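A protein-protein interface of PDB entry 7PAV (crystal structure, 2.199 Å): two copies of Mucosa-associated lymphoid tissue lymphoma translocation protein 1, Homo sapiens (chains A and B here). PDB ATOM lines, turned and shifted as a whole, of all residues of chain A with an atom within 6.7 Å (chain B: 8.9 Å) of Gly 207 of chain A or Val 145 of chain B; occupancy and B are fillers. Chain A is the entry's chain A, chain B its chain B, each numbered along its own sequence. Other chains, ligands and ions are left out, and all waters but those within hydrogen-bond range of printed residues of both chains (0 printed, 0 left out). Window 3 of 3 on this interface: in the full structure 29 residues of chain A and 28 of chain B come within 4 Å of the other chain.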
ATOM      1  N   THR A 155      30.051 -23.459  15.494  1.00  0.00           N
ATOM      2  CA  THR A 155      28.773 -22.963  15.004  1.00  0.00           C
ATOM      3  C   THR A 155      27.600 -23.931  15.347  1.00  0.00           C
ATOM      4  O   THR A 155      27.813 -25.003  15.906  1.00  0.00           O
ATOM      5  CB  THR A 155      28.899 -22.637  13.492  1.00  0.00           C
ATOM      6  OG1 THR A 155      27.691 -21.993  13.071  1.00  0.00           O
ATOM      7  CG2 THR A 155      29.207 -23.884  12.621  1.00  0.00           C
ATOM      8  N   CYS A 156      26.368 -23.523  15.056  1.00  0.00           N
ATOM      9  CA  CYS A 156      25.207 -24.363  15.239  1.00  0.00           C
ATOM     10  C   CYS A 156      25.054 -25.312  14.037  1.00  0.00           C
ATOM     11  O   CYS A 156      25.721 -25.143  13.006  1.00  0.00           O
ATOM     12  CB  CYS A 156      23.960 -23.516  15.465  1.00  0.00           C
ATOM     13  SG  CYS A 156      23.896 -22.737  17.096  1.00  0.00           S
ATOM     14  N   ALA A 159      24.691 -24.631   9.918  1.00  0.00           N
ATOM     15  CA  ALA A 159      25.186 -23.275   9.709  1.00  0.00           C
ATOM     16  C   ALA A 159      26.676 -23.283   9.303  1.00  0.00           C
ATOM     17  O   ALA A 159      27.367 -24.291   9.509  1.00  0.00           O
ATOM     18  CB  ALA A 159      24.987 -22.461  10.979  1.00  0.00           C
ATOM     19  N   MET A 199      30.486 -14.488  22.661  1.00  0.00           N
ATOM     20  CA  MET A 199      30.168 -14.387  21.240  1.00  0.00           C
ATOM     21  C   MET A 199      28.818 -13.725  21.000  1.00  0.00           C
ATOM     22  O   MET A 199      28.639 -13.040  20.001  1.00  0.00           O
ATOM     23  CB  MET A 199      30.163 -15.758  20.590  1.00  0.00           C
ATOM     24  CG  MET A 199      31.508 -16.247  20.236  1.00  0.00           C
ATOM     25  SD  MET A 199      31.443 -17.771  19.285  1.00  0.00           S
ATOM     26  CE  MET A 199      30.506 -17.251  17.898  1.00  0.00           C
ATOM     27  N   GLY A 200      27.874 -13.951  21.896  1.00  0.00           N
ATOM     28  CA  GLY A 200      26.560 -13.345  21.794  1.00  0.00           C
ATOM     29  C   GLY A 200      26.575 -11.882  22.168  1.00  0.00           C
ATOM     30  O   GLY A 200      25.753 -11.116  21.674  1.00  0.00           O
ATOM     31  N   CYS A 202      29.242  -9.769  21.691  1.00  0.00           N
ATOM     32  CA  CYS A 202      29.946  -9.026  20.660  1.00  0.00           C
ATOM     33  C   CYS A 202      29.080  -8.707  19.448  1.00  0.00           C
ATOM     34  O   CYS A 202      28.531  -9.599  18.814  1.00  0.00           O
ATOM     35  CB  CYS A 202      31.235  -9.732  20.263  1.00  0.00           C
ATOM     36  SG  CYS A 202      32.221  -8.838  19.036  1.00  0.00           S
ATOM     37  N   HIS A 203      28.984  -7.412  19.134  1.00  0.00           N
ATOM     38  CA  HIS A 203      28.208  -6.822  18.040  1.00  0.00           C
ATOM     39  C   HIS A 203      28.412  -7.473  16.646  1.00  0.00           C
ATOM     40  O   HIS A 203      27.418  -7.769  15.970  1.00  0.00           O
ATOM     41  CB  HIS A 203      28.473  -5.300  17.965  1.00  0.00           C
ATOM     42  CG  HIS A 203      29.904  -4.937  17.698  1.00  0.00           C
ATOM     43  ND1 HIS A 203      30.264  -4.186  16.587  1.00  0.00           N
ATOM     44  CD2 HIS A 203      31.028  -5.268  18.382  1.00  0.00           C
ATOM     45  CE1 HIS A 203      31.585  -4.085  16.632  1.00  0.00           C
ATOM     46  NE2 HIS A 203      32.091  -4.723  17.692  1.00  0.00           N
ATOM     47  N   LEU A 204      29.666  -7.727  16.235  1.00  0.00           N
ATOM     48  CA  LEU A 204      29.923  -8.261  14.900  1.00  0.00           C
ATOM     49  C   LEU A 204      29.817  -9.778  14.759  1.00  0.00           C
ATOM     50  O   LEU A 204      30.014 -10.294  13.657  1.00  0.00           O
ATOM     51  CB  LEU A 204      31.271  -7.774  14.363  1.00  0.00           C
ATOM     52  CG  LEU A 204      31.173  -6.691  13.273  1.00  0.00           C
ATOM     53  CD1 LEU A 204      30.491  -7.237  12.025  1.00  0.00           C
ATOM     54  CD2 LEU A 204      30.438  -5.428  13.780  1.00  0.00           C
ATOM     55  N   THR A 205      29.478 -10.491  15.837  1.00  0.00           N
ATOM     56  CA  THR A 205      29.311 -11.950  15.773  1.00  0.00           C
ATOM     57  C   THR A 205      27.886 -12.380  16.208  1.00  0.00           C
ATOM     58  O   THR A 205      27.433 -13.453  15.816  1.00  0.00           O
ATOM     59  CB  THR A 205      30.448 -12.693  16.518  1.00  0.00           C
ATOM     60  OG1 THR A 205      30.094 -14.055  16.731  1.00  0.00           O
ATOM     61  CG2 THR A 205      30.801 -12.070  17.832  1.00  0.00           C
ATOM     62  N   LYS A 206      27.190 -11.550  16.993  1.00  0.00           N
ATOM     63  CA  LYS A 206      25.829 -11.804  17.460  1.00  0.00           C
ATOM     64  C   LYS A 206      24.860 -11.928  16.271  1.00  0.00           C
ATOM     65  O   LYS A 206      24.741 -11.005  15.460  1.00  0.00           O
ATOM     66  CB  LYS A 206      25.409 -10.670  18.415  1.00  0.00           C
ATOM     67  CG  LYS A 206      23.924 -10.517  18.677  1.00  0.00           C
ATOM     68  CD  LYS A 206      23.650  -9.358  19.625  1.00  0.00           C
ATOM     69  CE  LYS A 206      24.138  -8.028  19.099  1.00  0.00           C
ATOM     70  NZ  LYS A 206      23.666  -7.756  17.710  1.00  0.00           N
ATOM     71  N   GLY A 207      24.195 -13.073  16.172  1.00  0.00           N
ATOM     72  CA  GLY A 207      23.257 -13.341  15.089  1.00  0.00           C
ATOM     73  C   GLY A 207      23.870 -14.121  13.938  1.00  0.00           C
ATOM     74  O   GLY A 207      23.208 -14.984  13.353  1.00  0.00           O
ATOM     75  N   LYS A 208      25.142 -13.829  13.597  1.00  0.00           N
ATOM     76  CA  LYS A 208      25.836 -14.509  12.497  1.00  0.00           C
ATOM     77  C   LYS A 208      26.450 -15.872  12.894  1.00  0.00           C
ATOM     78  O   LYS A 208      26.401 -16.819  12.105  1.00  0.00           O
ATOM     79  CB  LYS A 208      26.901 -13.592  11.859  1.00  0.00           C
ATOM     80  CG  LYS A 208      26.338 -12.318  11.216  1.00  0.00           C
ATOM     81  CD  LYS A 208      25.373 -12.608  10.061  1.00  0.00           C
ATOM     82  CE  LYS A 208      24.948 -11.345   9.350  1.00  0.00           C
ATOM     83  NZ  LYS A 208      23.584 -11.477   8.760  1.00  0.00           N
ATOM     84  N   GLN A 209      27.043 -15.970  14.091  1.00  0.00           N
ATOM     85  CA  GLN A 209      27.627 -17.233  14.549  1.00  0.00           C
ATOM     86  C   GLN A 209      27.377 -17.443  16.036  1.00  0.00           C
ATOM     87  O   GLN A 209      27.482 -16.503  16.830  1.00  0.00           O
ATOM     88  CB  GLN A 209      29.125 -17.302  14.226  1.00  0.00           C
ATOM     89  CG  GLN A 209      29.771 -18.664  14.488  1.00  0.00           C
ATOM     90  CD  GLN A 209      31.101 -18.761  13.777  1.00  0.00           C
ATOM     91  OE1 GLN A 209      31.279 -18.224  12.676  1.00  0.00           O
ATOM     92  NE2 GLN A 209      32.065 -19.445  14.380  1.00  0.00           N
ATOM     93  N   ALA A 210      27.007 -18.664  16.409  1.00  0.00           N
ATOM     94  CA  ALA A 210      26.753 -18.992  17.805  1.00  0.00           C
ATOM     95  C   ALA A 210      27.403 -20.311  18.148  1.00  0.00           C
ATOM     96  O   ALA A 210      27.322 -21.240  17.361  1.00  0.00           O
ATOM     97  CB  ALA A 210      25.252 -19.063  18.073  1.00  0.00           C
ATOM     98  N   LYS B 110      11.549 -25.636  15.316  1.00  0.00           N
ATOM     99  CA  LYS B 110      11.491 -24.666  14.232  1.00  0.00           C
ATOM    100  C   LYS B 110      10.226 -23.828  14.236  1.00  0.00           C
ATOM    101  O   LYS B 110      10.291 -22.637  13.948  1.00  0.00           O
ATOM    102  CB  LYS B 110      11.714 -25.336  12.870  1.00  0.00           C
ATOM    103  CG  LYS B 110      13.126 -25.882  12.700  1.00  0.00           C
ATOM    104  CD  LYS B 110      13.599 -25.833  11.229  1.00  0.00           C
ATOM    105  CE  LYS B 110      14.180 -24.491  10.803  1.00  0.00           C
ATOM    106  NZ  LYS B 110      14.222 -24.348   9.323  1.00  0.00           N
ATOM    107  N   GLN B 113      10.556 -21.085  16.861  1.00  0.00           N
ATOM    108  CA  GLN B 113      11.471 -20.064  16.352  1.00  0.00           C
ATOM    109  C   GLN B 113      10.762 -19.045  15.450  1.00  0.00           C
ATOM    110  O   GLN B 113      11.163 -17.878  15.393  1.00  0.00           O
ATOM    111  CB  GLN B 113      12.646 -20.723  15.603  1.00  0.00           C
ATOM    112  CG  GLN B 113      13.533 -21.558  16.509  1.00  0.00           C
ATOM    113  CD  GLN B 113      14.685 -22.161  15.751  1.00  0.00           C
ATOM    114  OE1 GLN B 113      14.672 -23.341  15.380  1.00  0.00           O
ATOM    115  NE2 GLN B 113      15.709 -21.367  15.508  1.00  0.00           N
ATOM    116  N   ASN B 120      14.002 -21.177  24.482  1.00  0.00           N
ATOM    117  CA  ASN B 120      13.293 -22.411  24.166  1.00  0.00           C
ATOM    118  C   ASN B 120      13.997 -23.496  24.930  1.00  0.00           C
ATOM    119  O   ASN B 120      15.178 -23.727  24.689  1.00  0.00           O
ATOM    120  CB  ASN B 120      13.356 -22.728  22.680  1.00  0.00           C
ATOM    121  CG  ASN B 120      12.991 -21.573  21.777  1.00  0.00           C
ATOM    122  OD1 ASN B 120      11.829 -21.329  21.461  1.00  0.00           O
ATOM    123  ND2 ASN B 120      13.988 -20.836  21.314  1.00  0.00           N
ATOM    124  N   ALA B 142      17.010 -27.595   8.653  1.00  0.00           N
ATOM    125  CA  ALA B 142      17.296 -27.332  10.044  1.00  0.00           C
ATOM    126  C   ALA B 142      18.065 -26.047  10.297  1.00  0.00           C
ATOM    127  O   ALA B 142      18.718 -25.503   9.393  1.00  0.00           O
ATOM    128  CB  ALA B 142      18.023 -28.538  10.649  1.00  0.00           C
ATOM    129  N   LEU B 143      17.898 -25.530  11.522  1.00  0.00           N
ATOM    130  CA  LEU B 143      18.551 -24.354  12.050  1.00  0.00           C
ATOM    131  C   LEU B 143      18.042 -23.023  11.526  1.00  0.00           C
ATOM    132  O   LEU B 143      17.532 -22.874  10.414  1.00  0.00           O
ATOM    133  CB  LEU B 143      20.078 -24.425  11.876  1.00  0.00           C
ATOM    134  N   LYS B 144      18.179 -22.071  12.420  1.00  0.00           N
ATOM    135  CA  LYS B 144      18.021 -20.637  12.372  1.00  0.00           C
ATOM    136  C   LYS B 144      18.768 -20.260  13.648  1.00  0.00           C
ATOM    137  O   LYS B 144      18.415 -20.732  14.737  1.00  0.00           O
ATOM    138  CB  LYS B 144      16.548 -20.183  12.391  1.00  0.00           C
ATOM    139  CG  LYS B 144      16.352 -18.768  11.827  1.00  0.00           C
ATOM    140  CD  LYS B 144      16.812 -18.656  10.352  1.00  0.00           C
ATOM    141  CE  LYS B 144      17.906 -17.627  10.113  1.00  0.00           C
ATOM    142  NZ  LYS B 144      19.164 -17.968  10.833  1.00  0.00           N
ATOM    143  N   VAL B 145      19.904 -19.574  13.496  1.00  0.00           N
ATOM    144  CA  VAL B 145      20.743 -19.228  14.638  1.00  0.00           C
ATOM    145  C   VAL B 145      20.056 -18.137  15.485  1.00  0.00           C
ATOM    146  O   VAL B 145      20.228 -16.932  15.282  1.00  0.00           O
ATOM    147  CB  VAL B 145      22.229 -18.925  14.260  1.00  0.00           C
ATOM    148  CG1 VAL B 145      22.356 -18.187  12.926  1.00  0.00           C
ATOM    149  CG2 VAL B 145      22.970 -18.197  15.378  1.00  0.00           C
ATOM    150  N   THR B 146      19.183 -18.603  16.382  1.00  0.00           N
ATOM    151  CA  THR B 146      18.459 -17.766  17.330  1.00  0.00           C
ATOM    152  C   THR B 146      19.242 -17.631  18.650  1.00  0.00           C
ATOM    153  O   THR B 146      18.983 -16.676  19.402  1.00  0.00           O
ATOM    154  CB  THR B 146      17.003 -18.239  17.514  1.00  0.00           C
ATOM    155  OG1 THR B 146      16.962 -19.625  17.881  1.00  0.00           O
ATOM    156  CG2 THR B 146      16.158 -17.996  16.283  1.00  0.00           C
ATOM    157  N   ALA B 147      20.204 -18.579  18.906  1.00  0.00           N
ATOM    158  CA  ALA B 147      21.103 -18.665  20.045  1.00  0.00           C
ATOM    159  C   ALA B 147      20.338 -18.605  21.352  1.00  0.00           C
ATOM    160  O   ALA B 147      20.680 -17.849  22.263  1.00  0.00           O
ATOM    161  CB  ALA B 147      22.167 -17.573  19.969  1.00  0.00           C
ATOM    162  N   ASN B 148      19.283 -19.404  21.432  1.00  0.00           N
ATOM    163  CA  ASN B 148      18.415 -19.411  22.604  1.00  0.00           C
ATOM    164  C   ASN B 148      17.779 -20.770  22.869  1.00  0.00           C
ATOM    165  O   ASN B 148      16.741 -20.804  23.508  1.00  0.00           O
ATOM    166  CB  ASN B 148      17.312 -18.350  22.425  1.00  0.00           C
ATOM    167  CG  ASN B 148      16.387 -18.549  21.220  1.00  0.00           C
ATOM    168  OD1 ASN B 148      15.523 -17.707  20.920  1.00  0.00           O
ATOM    169  ND2 ASN B 148      16.508 -19.669  20.502  1.00  0.00           N
ATOM    170  N   ILE B 149      18.354 -21.868  22.369  1.00  0.00           N
ATOM    171  CA  ILE B 149      17.773 -23.190  22.549  1.00  0.00           C
ATOM    172  C   ILE B 149      18.571 -24.037  23.505  1.00  0.00           C
ATOM    173  O   ILE B 149      19.743 -24.274  23.253  1.00  0.00           O
ATOM    174  CB  ILE B 149      17.662 -23.939  21.200  1.00  0.00           C
ATOM    175  CG1 ILE B 149      17.036 -23.085  20.098  1.00  0.00           C
ATOM    176  CG2 ILE B 149      16.941 -25.273  21.341  1.00  0.00           C
ATOM    177  CD1 ILE B 149      17.672 -23.412  18.694  1.00  0.00           C
ATOM    178  N   SER B 216      22.666 -23.839  22.697  1.00  0.00           N
ATOM    179  CA  SER B 216      23.172 -22.741  21.901  1.00  0.00           C
ATOM    180  C   SER B 216      22.824 -21.382  22.534  1.00  0.00           C
ATOM    181  O   SER B 216      23.001 -20.372  21.880  1.00  0.00           O
ATOM    182  CB  SER B 216      22.670 -22.817  20.465  1.00  0.00           C
ATOM    183  OG  SER B 216      21.300 -22.474  20.372  1.00  0.00           O
ATOM    184  N   SER B 218      23.167 -17.997  24.230  1.00  0.00           N
ATOM    185  CA  SER B 218      24.264 -17.037  24.318  1.00  0.00           C
ATOM    186  C   SER B 218      23.990 -15.896  25.321  1.00  0.00           C
ATOM    187  O   SER B 218      24.726 -14.910  25.315  1.00  0.00           O
ATOM    188  CB  SER B 218      24.536 -16.443  22.942  1.00  0.00           C
ATOM    189  OG  SER B 218      23.388 -15.731  22.519  1.00  0.00           O
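Of the 13 printed residues of chain B, 4 touch a printed residue of chain A. Hydrophobic or aromatic side chains of chain A that line the printed part of chain B: Ala 210. Among the printed residues, 5 pairs touch across the chains. Among the printed residues, no Asp or Glu carboxylate lies within 4 Å of a Lys or Arg side-chain nitrogen of the other chain.
No position is printed for both chains. Of the 5 pairs that touch across the chains among the printed residues, none has its exchanged pair printed and touching as well.
Of the printed residues of chain B, Gly 200 of chain A touches Ser 218 (3.9 Å). Cys 202 of chain A touches none of the printed residues of chain B. Gly 207 of chain A touches just one residue of chain B: Val 145. Asn 120 of chain B touches none of the printed residues of chain A. Of the printed residues of chain A, Ser 218 of chain B touches Gly 200. The nearest residue of chain A that does not touch Val 145 of chain B is Lys 208 of chain A (4.3 Å). The nearest printed residue of chain B that does not touch Ala 210 of chain A is Ser 216 of chain B (4.6 Å).
SG of Cys 156 of chain A touches CB of Ser 216 of chain B (3.6 Å). Gly 200 of chain A touches Ser 218 of chain B (CA to CB, 3.9 Å). Val 145 of chain B touches Gly 207 of chain A (CG1 to O, 3.3 Å). CG2 of Val 145 of chain B touches CB of Ala 210 of chain A, 3.6 Å away. CB of Ala 147 of chain B touches CB of Ala 210 of chain A (3.9 Å).
O of Ala 147 of chain B is in hydrogen-bond range of N of Ser 218 of chain B (3.2 Å). The backbone carbonyl oxygen of Ile 149 of chain B sits at hydrogen-bond distance from the backbone NH of Ser 216 of chain B. The backbone carbonyl oxygen of Ala 210 of chain A is in hydrogen-bond range of the backbone NH of Cys 156 of chain A (3.4 Å).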
